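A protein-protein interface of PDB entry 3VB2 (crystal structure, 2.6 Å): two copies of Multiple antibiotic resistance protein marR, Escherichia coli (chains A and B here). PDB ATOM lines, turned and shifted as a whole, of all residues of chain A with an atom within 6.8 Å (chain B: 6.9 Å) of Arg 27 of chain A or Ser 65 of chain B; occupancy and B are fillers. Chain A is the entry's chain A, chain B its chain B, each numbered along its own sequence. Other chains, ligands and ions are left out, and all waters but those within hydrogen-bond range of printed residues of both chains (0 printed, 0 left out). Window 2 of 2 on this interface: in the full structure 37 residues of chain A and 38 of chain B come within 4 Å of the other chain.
Leu 143 of chain B touches Met 20 of chain A. Ser 65 of chain B touches Arg 27 of chain A.
No position is printed for both chains. Of the 4 pairs that touch across the chains among the printed residues, none has its exchanged pair printed and touching as well.
Hydrophobic or aromatic side chains of chain B within 4 Å of the printed part of chain A: Leu 143. Of the 15 printed residues of chain A, 3 touch a printed residue of chain B. Printed residues of chain A that touch a printed residue of chain B: Met 20, Gln 23 and Arg 27. Hydrophobic or aromatic side chains of chain A that line the printed part of chain B: Met 20. Among the printed residues, 4 pairs touch across the chains. Among the printed residues, no Asp or Glu carboxylate lies within 4 Å of a Lys or Arg side-chain nitrogen of the other chain.
O of Val 63 of chain B lies within hydrogen-bond range of NE2 of Gln 23 of chain A, at 3.4 Å. The backbone carbonyl oxygen of Leu 64 of chain B lies within hydrogen-bond range of the side-chain amide nitrogen of Gln 23 of chain A (3.3 Å).
Arg 27 of chain A touches just one residue of chain B: Ser 65 (3.7 Å). Of chain A, only Arg 27 (3.7 Å) comes within 4 Å of Ser 65 of chain B. Printed residues of chain A within 4 Å of Leu 143 of chain B: Met 20. Of the printed residues of chain A, Val 63 of chain B touches Gln 23. Printed residues of chain A within 4 Å of Leu 64 of chain B: Gln 23. Leu 119 of chain A touches none of the printed residues of chain B. The nearest residue of chain B that does not touch Arg 27 of chain A is Val 63 of chain B (5.3 Å). The nearest residue of chain A that does not touch Ser 65 of chain B is Gln 23 of chain A (4.6 Å). The nearest printed residue of chain B that does not touch Gln 23 of chain A is Ser 65 of chain B (4.6 Å).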
ATOM      1  N   MET A  20      -7.681   5.384 -26.371  1.00  0.00           N
ATOM      2  CA  MET A  20      -8.038   3.984 -26.091  1.00  0.00           C
ATOM      3  C   MET A  20      -7.680   3.538 -24.668  1.00  0.00           C
ATOM      4  O   MET A  20      -8.450   2.822 -24.024  1.00  0.00           O
ATOM      5  CB  MET A  20      -7.380   3.059 -27.098  1.00  0.00           C
ATOM      6  CG  MET A  20      -8.006   3.106 -28.464  1.00  0.00           C
ATOM      7  SD  MET A  20      -6.908   2.452 -29.693  1.00  0.00           S
ATOM      8  CE  MET A  20      -7.270   0.707 -29.579  1.00  0.00           C
ATOM      9  N   ASN A  22      -7.276   5.627 -22.110  1.00  0.00           N
ATOM     10  CA  ASN A  22      -8.156   6.381 -21.282  1.00  0.00           C
ATOM     11  C   ASN A  22      -9.585   5.802 -21.226  1.00  0.00           C
ATOM     12  O   ASN A  22     -10.196   5.788 -20.174  1.00  0.00           O
ATOM     13  CB  ASN A  22      -8.183   7.821 -21.716  1.00  0.00           C
ATOM     14  CG  ASN A  22      -8.967   8.688 -20.775  1.00  0.00           C
ATOM     15  OD1 ASN A  22      -8.480   9.062 -19.696  1.00  0.00           O
ATOM     16  ND2 ASN A  22     -10.191   9.009 -21.157  1.00  0.00           N
ATOM     17  N   GLN A  23     -10.098   5.329 -22.379  1.00  0.00           N
ATOM     18  CA  GLN A  23     -11.364   4.581 -22.413  1.00  0.00           C
ATOM     19  C   GLN A  23     -11.315   3.348 -21.509  1.00  0.00           C
ATOM     20  O   GLN A  23     -12.280   3.037 -20.825  1.00  0.00           O
ATOM     21  CB  GLN A  23     -11.718   4.151 -23.854  1.00  0.00           C
ATOM     22  CG  GLN A  23     -12.198   5.277 -24.755  1.00  0.00           C
ATOM     23  CD  GLN A  23     -13.617   5.738 -24.430  1.00  0.00           C
ATOM     24  OE1 GLN A  23     -13.824   6.574 -23.545  1.00  0.00           O
ATOM     25  NE2 GLN A  23     -14.597   5.228 -25.184  1.00  0.00           N
ATOM     26  N   LYS A  24     -10.199   2.629 -21.551  1.00  0.00           N
ATOM     27  CA  LYS A  24     -10.068   1.369 -20.814  1.00  0.00           C
ATOM     28  C   LYS A  24     -10.060   1.632 -19.317  1.00  0.00           C
ATOM     29  O   LYS A  24     -10.705   0.917 -18.549  1.00  0.00           O
ATOM     30  CB  LYS A  24      -8.783   0.622 -21.241  1.00  0.00           C
ATOM     31  CG  LYS A  24      -8.515  -0.660 -20.476  1.00  0.00           C
ATOM     32  CD  LYS A  24      -7.274  -1.348 -21.007  1.00  0.00           C
ATOM     33  CE  LYS A  24      -6.668  -2.314 -19.982  1.00  0.00           C
ATOM     34  NZ  LYS A  24      -7.528  -3.499 -19.745  1.00  0.00           N
ATOM     35  N   LYS A  25      -9.329   2.674 -18.909  1.00  0.00           N
ATOM     36  CA  LYS A  25      -9.343   3.143 -17.520  1.00  0.00           C
ATOM     37  C   LYS A  25     -10.766   3.497 -17.052  1.00  0.00           C
ATOM     38  O   LYS A  25     -11.182   3.101 -15.956  1.00  0.00           O
ATOM     39  CB  LYS A  25      -8.399   4.361 -17.337  1.00  0.00           C
ATOM     40  CG  LYS A  25      -8.571   5.080 -15.989  1.00  0.00           C
ATOM     41  CD  LYS A  25      -7.862   6.430 -15.951  1.00  0.00           C
ATOM     42  CE  LYS A  25      -8.468   7.426 -16.949  1.00  0.00           C
ATOM     43  NZ  LYS A  25      -9.482   8.344 -16.343  1.00  0.00           N
ATOM     44  N   ASP A  26     -11.506   4.222 -17.900  1.00  0.00           N
ATOM     45  CA  ASP A  26     -12.881   4.651 -17.580  1.00  0.00           C
ATOM     46  C   ASP A  26     -13.848   3.489 -17.454  1.00  0.00           C
ATOM     47  O   ASP A  26     -14.758   3.529 -16.626  1.00  0.00           O
ATOM     48  CB  ASP A  26     -13.396   5.667 -18.607  1.00  0.00           C
ATOM     49  CG  ASP A  26     -12.912   7.096 -18.317  1.00  0.00           C
ATOM     50  OD1 ASP A  26     -12.161   7.305 -17.324  1.00  0.00           O
ATOM     51  OD2 ASP A  26     -13.265   8.000 -19.083  1.00  0.00           O
ATOM     52  N   ARG A  27     -13.639   2.445 -18.270  1.00  0.00           N
ATOM     53  CA  ARG A  27     -14.460   1.238 -18.201  1.00  0.00           C
ATOM     54  C   ARG A  27     -14.175   0.456 -16.923  1.00  0.00           C
ATOM     55  O   ARG A  27     -15.092  -0.002 -16.258  1.00  0.00           O
ATOM     56  CB  ARG A  27     -14.250   0.351 -19.439  1.00  0.00           C
ATOM     57  CG  ARG A  27     -14.960   0.847 -20.691  1.00  0.00           C
ATOM     58  CD  ARG A  27     -15.110  -0.265 -21.731  1.00  0.00           C
ATOM     59  NE  ARG A  27     -13.819  -0.875 -22.083  1.00  0.00           N
ATOM     60  CZ  ARG A  27     -12.939  -0.344 -22.942  1.00  0.00           C
ATOM     61  NH1 ARG A  27     -13.210   0.802 -23.552  1.00  0.00           N
ATOM     62  NH2 ARG A  27     -11.784  -0.965 -23.185  1.00  0.00           N
ATOM     63  N   LEU A  28     -12.900   0.369 -16.551  1.00  0.00           N
ATOM     64  CA  LEU A  28     -12.516  -0.282 -15.283  1.00  0.00           C
ATOM     65  C   LEU A  28     -13.057   0.486 -14.049  1.00  0.00           C
ATOM     66  O   LEU A  28     -13.673  -0.109 -13.154  1.00  0.00           O
ATOM     67  CB  LEU A  28     -10.997  -0.457 -15.200  1.00  0.00           C
ATOM     68  CG  LEU A  28     -10.388  -1.425 -16.224  1.00  0.00           C
ATOM     69  CD1 LEU A  28      -8.872  -1.268 -16.291  1.00  0.00           C
ATOM     70  CD2 LEU A  28     -10.774  -2.855 -15.888  1.00  0.00           C
ATOM     71  N   LEU A  29     -12.878   1.810 -14.050  1.00  0.00           N
ATOM     72  CA  LEU A  29     -13.535   2.697 -13.062  1.00  0.00           C
ATOM     73  C   LEU A  29     -15.041   2.442 -12.946  1.00  0.00           C
ATOM     74  O   LEU A  29     -15.558   2.211 -11.855  1.00  0.00           O
ATOM     75  CB  LEU A  29     -13.286   4.164 -13.407  1.00  0.00           C
ATOM     76  CG  LEU A  29     -12.059   4.801 -12.772  1.00  0.00           C
ATOM     77  CD1 LEU A  29     -12.082   6.309 -12.966  1.00  0.00           C
ATOM     78  CD2 LEU A  29     -11.976   4.450 -11.293  1.00  0.00           C
ATOM     79  N   ASN A  30     -15.739   2.509 -14.073  1.00  0.00           N
ATOM     80  CA  ASN A  30     -17.169   2.258 -14.096  1.00  0.00           C
ATOM     81  C   ASN A  30     -17.565   0.900 -13.490  1.00  0.00           C
ATOM     82  O   ASN A  30     -18.582   0.798 -12.817  1.00  0.00           O
ATOM     83  CB  ASN A  30     -17.729   2.420 -15.519  1.00  0.00           C
ATOM     84  CG  ASN A  30     -17.979   3.891 -15.888  1.00  0.00           C
ATOM     85  OD1 ASN A  30     -18.623   4.626 -15.151  1.00  0.00           O
ATOM     86  ND2 ASN A  30     -17.478   4.304 -17.018  1.00  0.00           N
ATOM     87  N   GLU A  31     -16.717  -0.117 -13.689  1.00  0.00           N
ATOM     88  CA  GLU A  31     -16.960  -1.451 -13.110  1.00  0.00           C
ATOM     89  C   GLU A  31     -16.778  -1.455 -11.603  1.00  0.00           C
ATOM     90  O   GLU A  31     -17.611  -1.973 -10.880  1.00  0.00           O
ATOM     91  CB  GLU A  31     -16.041  -2.480 -13.731  1.00  0.00           C
ATOM     92  CG  GLU A  31     -16.421  -2.896 -15.124  1.00  0.00           C
ATOM     93  CD  GLU A  31     -15.447  -3.898 -15.694  1.00  0.00           C
ATOM     94  OE1 GLU A  31     -15.100  -4.868 -14.972  1.00  0.00           O
ATOM     95  OE2 GLU A  31     -14.999  -3.708 -16.849  1.00  0.00           O
ATOM     96  N   TYR A  32     -15.662  -0.893 -11.142  1.00  0.00           N
ATOM     97  CA  TYR A  32     -15.333  -0.899  -9.731  1.00  0.00           C
ATOM     98  C   TYR A  32     -16.258   0.024  -8.966  1.00  0.00           C
ATOM     99  O   TYR A  32     -16.564  -0.222  -7.816  1.00  0.00           O
ATOM    100  CB  TYR A  32     -13.858  -0.496  -9.497  1.00  0.00           C
ATOM    101  CG  TYR A  32     -12.837  -1.378 -10.213  1.00  0.00           C
ATOM    102  CD1 TYR A  32     -12.920  -2.773 -10.155  1.00  0.00           C
ATOM    103  CD2 TYR A  32     -11.780  -0.815 -10.910  1.00  0.00           C
ATOM    104  CE1 TYR A  32     -11.996  -3.574 -10.809  1.00  0.00           C
ATOM    105  CE2 TYR A  32     -10.849  -1.606 -11.567  1.00  0.00           C
ATOM    106  CZ  TYR A  32     -10.961  -2.985 -11.513  1.00  0.00           C
ATOM    107  OH  TYR A  32     -10.032  -3.773 -12.165  1.00  0.00           O
ATOM    108  N   ALA A  40     -17.836   6.877 -13.603  1.00  0.00           N
ATOM    109  CA  ALA A  40     -16.494   7.483 -13.678  1.00  0.00           C
ATOM    110  C   ALA A  40     -16.577   8.998 -13.885  1.00  0.00           C
ATOM    111  O   ALA A  40     -15.863   9.756 -13.247  1.00  0.00           O
ATOM    112  CB  ALA A  40     -15.676   6.842 -14.784  1.00  0.00           C
ATOM    113  N   ALA A  41     -17.454   9.424 -14.784  1.00  0.00           N
ATOM    114  CA  ALA A  41     -17.707  10.846 -15.002  1.00  0.00           C
ATOM    115  C   ALA A  41     -18.089  11.589 -13.687  1.00  0.00           C
ATOM    116  O   ALA A  41     -17.517  12.637 -13.375  1.00  0.00           O
ATOM    117  CB  ALA A  41     -18.792  11.040 -16.070  1.00  0.00           C
ATOM    118  N   LEU A 119      -7.323  -0.011  -9.793  1.00  0.00           N
ATOM    119  CA  LEU A 119      -7.222   0.399 -11.174  1.00  0.00           C
ATOM    120  C   LEU A 119      -5.787   0.254 -11.670  1.00  0.00           C
ATOM    121  O   LEU A 119      -5.545  -0.298 -12.752  1.00  0.00           O
ATOM    122  CB  LEU A 119      -7.708   1.835 -11.347  1.00  0.00           C
ATOM    123  CG  LEU A 119      -7.635   2.410 -12.756  1.00  0.00           C
ATOM    124  CD1 LEU A 119      -8.850   1.980 -13.561  1.00  0.00           C
ATOM    125  CD2 LEU A 119      -7.531   3.934 -12.704  1.00  0.00           C
ATOM    126  N   LEU B  60     -24.224   2.896 -29.178  1.00  0.00           N
ATOM    127  CA  LEU B  60     -23.244   3.983 -29.241  1.00  0.00           C
ATOM    128  C   LEU B  60     -22.855   4.447 -27.846  1.00  0.00           C
ATOM    129  O   LEU B  60     -21.676   4.606 -27.543  1.00  0.00           O
ATOM    130  CB  LEU B  60     -23.807   5.155 -30.045  1.00  0.00           C
ATOM    131  CG  LEU B  60     -22.839   6.245 -30.484  1.00  0.00           C
ATOM    132  CD1 LEU B  60     -21.690   5.656 -31.299  1.00  0.00           C
ATOM    133  CD2 LEU B  60     -23.575   7.307 -31.285  1.00  0.00           C
ATOM    134  N   LYS B  61     -23.868   4.670 -26.996  1.00  0.00           N
ATOM    135  CA  LYS B  61     -23.644   4.973 -25.590  1.00  0.00           C
ATOM    136  C   LYS B  61     -22.629   4.001 -24.987  1.00  0.00           C
ATOM    137  O   LYS B  61     -21.665   4.419 -24.338  1.00  0.00           O
ATOM    138  CB  LYS B  61     -24.966   4.916 -24.816  1.00  0.00           C
ATOM    139  CG  LYS B  61     -24.811   4.804 -23.309  1.00  0.00           C
ATOM    140  CD  LYS B  61     -26.153   4.605 -22.634  1.00  0.00           C
ATOM    141  CE  LYS B  61     -26.524   3.131 -22.555  1.00  0.00           C
ATOM    142  NZ  LYS B  61     -25.893   2.464 -21.382  1.00  0.00           N
ATOM    143  N   LYS B  62     -22.829   2.706 -25.245  1.00  0.00           N
ATOM    144  CA  LYS B  62     -21.977   1.650 -24.670  1.00  0.00           C
ATOM    145  C   LYS B  62     -20.534   1.702 -25.199  1.00  0.00           C
ATOM    146  O   LYS B  62     -19.580   1.603 -24.424  1.00  0.00           O
ATOM    147  CB  LYS B  62     -22.589   0.261 -24.914  1.00  0.00           C
ATOM    148  CG  LYS B  62     -23.791  -0.046 -24.037  1.00  0.00           C
ATOM    149  CD  LYS B  62     -24.471  -1.340 -24.451  1.00  0.00           C
ATOM    150  CE  LYS B  62     -25.801  -1.509 -23.729  1.00  0.00           C
ATOM    151  NZ  LYS B  62     -26.290  -2.917 -23.757  1.00  0.00           N
ATOM    152  N   VAL B  63     -20.385   1.861 -26.515  1.00  0.00           N
ATOM    153  CA  VAL B  63     -19.054   2.003 -27.127  1.00  0.00           C
ATOM    154  C   VAL B  63     -18.296   3.230 -26.563  1.00  0.00           C
ATOM    155  O   VAL B  63     -17.100   3.159 -26.293  1.00  0.00           O
ATOM    156  CB  VAL B  63     -19.137   2.094 -28.687  1.00  0.00           C
ATOM    157  CG1 VAL B  63     -17.864   2.682 -29.257  1.00  0.00           C
ATOM    158  CG2 VAL B  63     -19.410   0.723 -29.294  1.00  0.00           C
ATOM    159  N   LEU B  64     -19.019   4.334 -26.363  1.00  0.00           N
ATOM    160  CA  LEU B  64     -18.404   5.610 -25.936  1.00  0.00           C
ATOM    161  C   LEU B  64     -18.254   5.707 -24.414  1.00  0.00           C
ATOM    162  O   LEU B  64     -17.421   6.462 -23.915  1.00  0.00           O
ATOM    163  CB  LEU B  64     -19.225   6.801 -26.449  1.00  0.00           C
ATOM    164  CG  LEU B  64     -19.169   7.111 -27.949  1.00  0.00           C
ATOM    165  CD1 LEU B  64     -20.324   8.032 -28.334  1.00  0.00           C
ATOM    166  CD2 LEU B  64     -17.822   7.718 -28.339  1.00  0.00           C
ATOM    167  N   SER B  65     -19.094   4.964 -23.687  1.00  0.00           N
ATOM    168  CA  SER B  65     -19.106   4.999 -22.218  1.00  0.00           C
ATOM    169  C   SER B  65     -19.561   6.361 -21.664  1.00  0.00           C
ATOM    170  O   SER B  65     -19.072   6.811 -20.627  1.00  0.00           O
ATOM    171  CB  SER B  65     -17.725   4.624 -21.648  1.00  0.00           C
ATOM    172  OG  SER B  65     -17.343   3.316 -22.044  1.00  0.00           O
ATOM    173  N   VAL B  66     -20.501   7.003 -22.359  1.00  0.00           N
ATOM    174  CA  VAL B  66     -21.089   8.265 -21.875  1.00  0.00           C
ATOM    175  C   VAL B  66     -22.631   8.163 -21.685  1.00  0.00           C
ATOM    176  O   VAL B  66     -23.267   7.234 -22.192  1.00  0.00           O
ATOM    177  CB  VAL B  66     -20.655   9.498 -22.766  1.00  0.00           C
ATOM    178  CG1 VAL B  66     -20.490   9.106 -24.219  1.00  0.00           C
ATOM    179  CG2 VAL B  66     -21.596  10.684 -22.595  1.00  0.00           C
ATOM    180  N   ASP B  67     -23.190   9.068 -20.870  1.00  0.00           N
ATOM    181  CA  ASP B  67     -24.628   9.045 -20.520  1.00  0.00           C
ATOM    182  C   ASP B  67     -25.527   9.059 -21.767  1.00  0.00           C
ATOM    183  O   ASP B  67     -25.246   9.771 -22.737  1.00  0.00           O
ATOM    184  CB  ASP B  67     -24.968  10.237 -19.619  1.00  0.00           C
ATOM    185  CG  ASP B  67     -26.336  10.110 -18.968  1.00  0.00           C
ATOM    186  OD1 ASP B  67     -26.435   9.457 -17.904  1.00  0.00           O
ATOM    187  OD2 ASP B  67     -27.305  10.688 -19.501  1.00  0.00           O
ATOM    188  N   LEU B 143      -3.430  -2.552 -23.494  1.00  0.00           N
ATOM    189  CA  LEU B 143      -4.770  -2.643 -24.119  1.00  0.00           C
ATOM    190  C   LEU B 143      -5.358  -4.068 -24.153  1.00  0.00           C
ATOM    191  O   LEU B 143      -6.592  -4.244 -24.087  1.00  0.00           O
ATOM    192  CB  LEU B 143      -4.759  -2.036 -25.518  1.00  0.00           C
ATOM    193  CG  LEU B 143      -4.712  -0.508 -25.582  1.00  0.00           C
ATOM    194  CD1 LEU B 143      -4.356  -0.041 -26.982  1.00  0.00           C
ATOM    195  CD2 LEU B 143      -6.040   0.089 -25.134  1.00  0.00           C
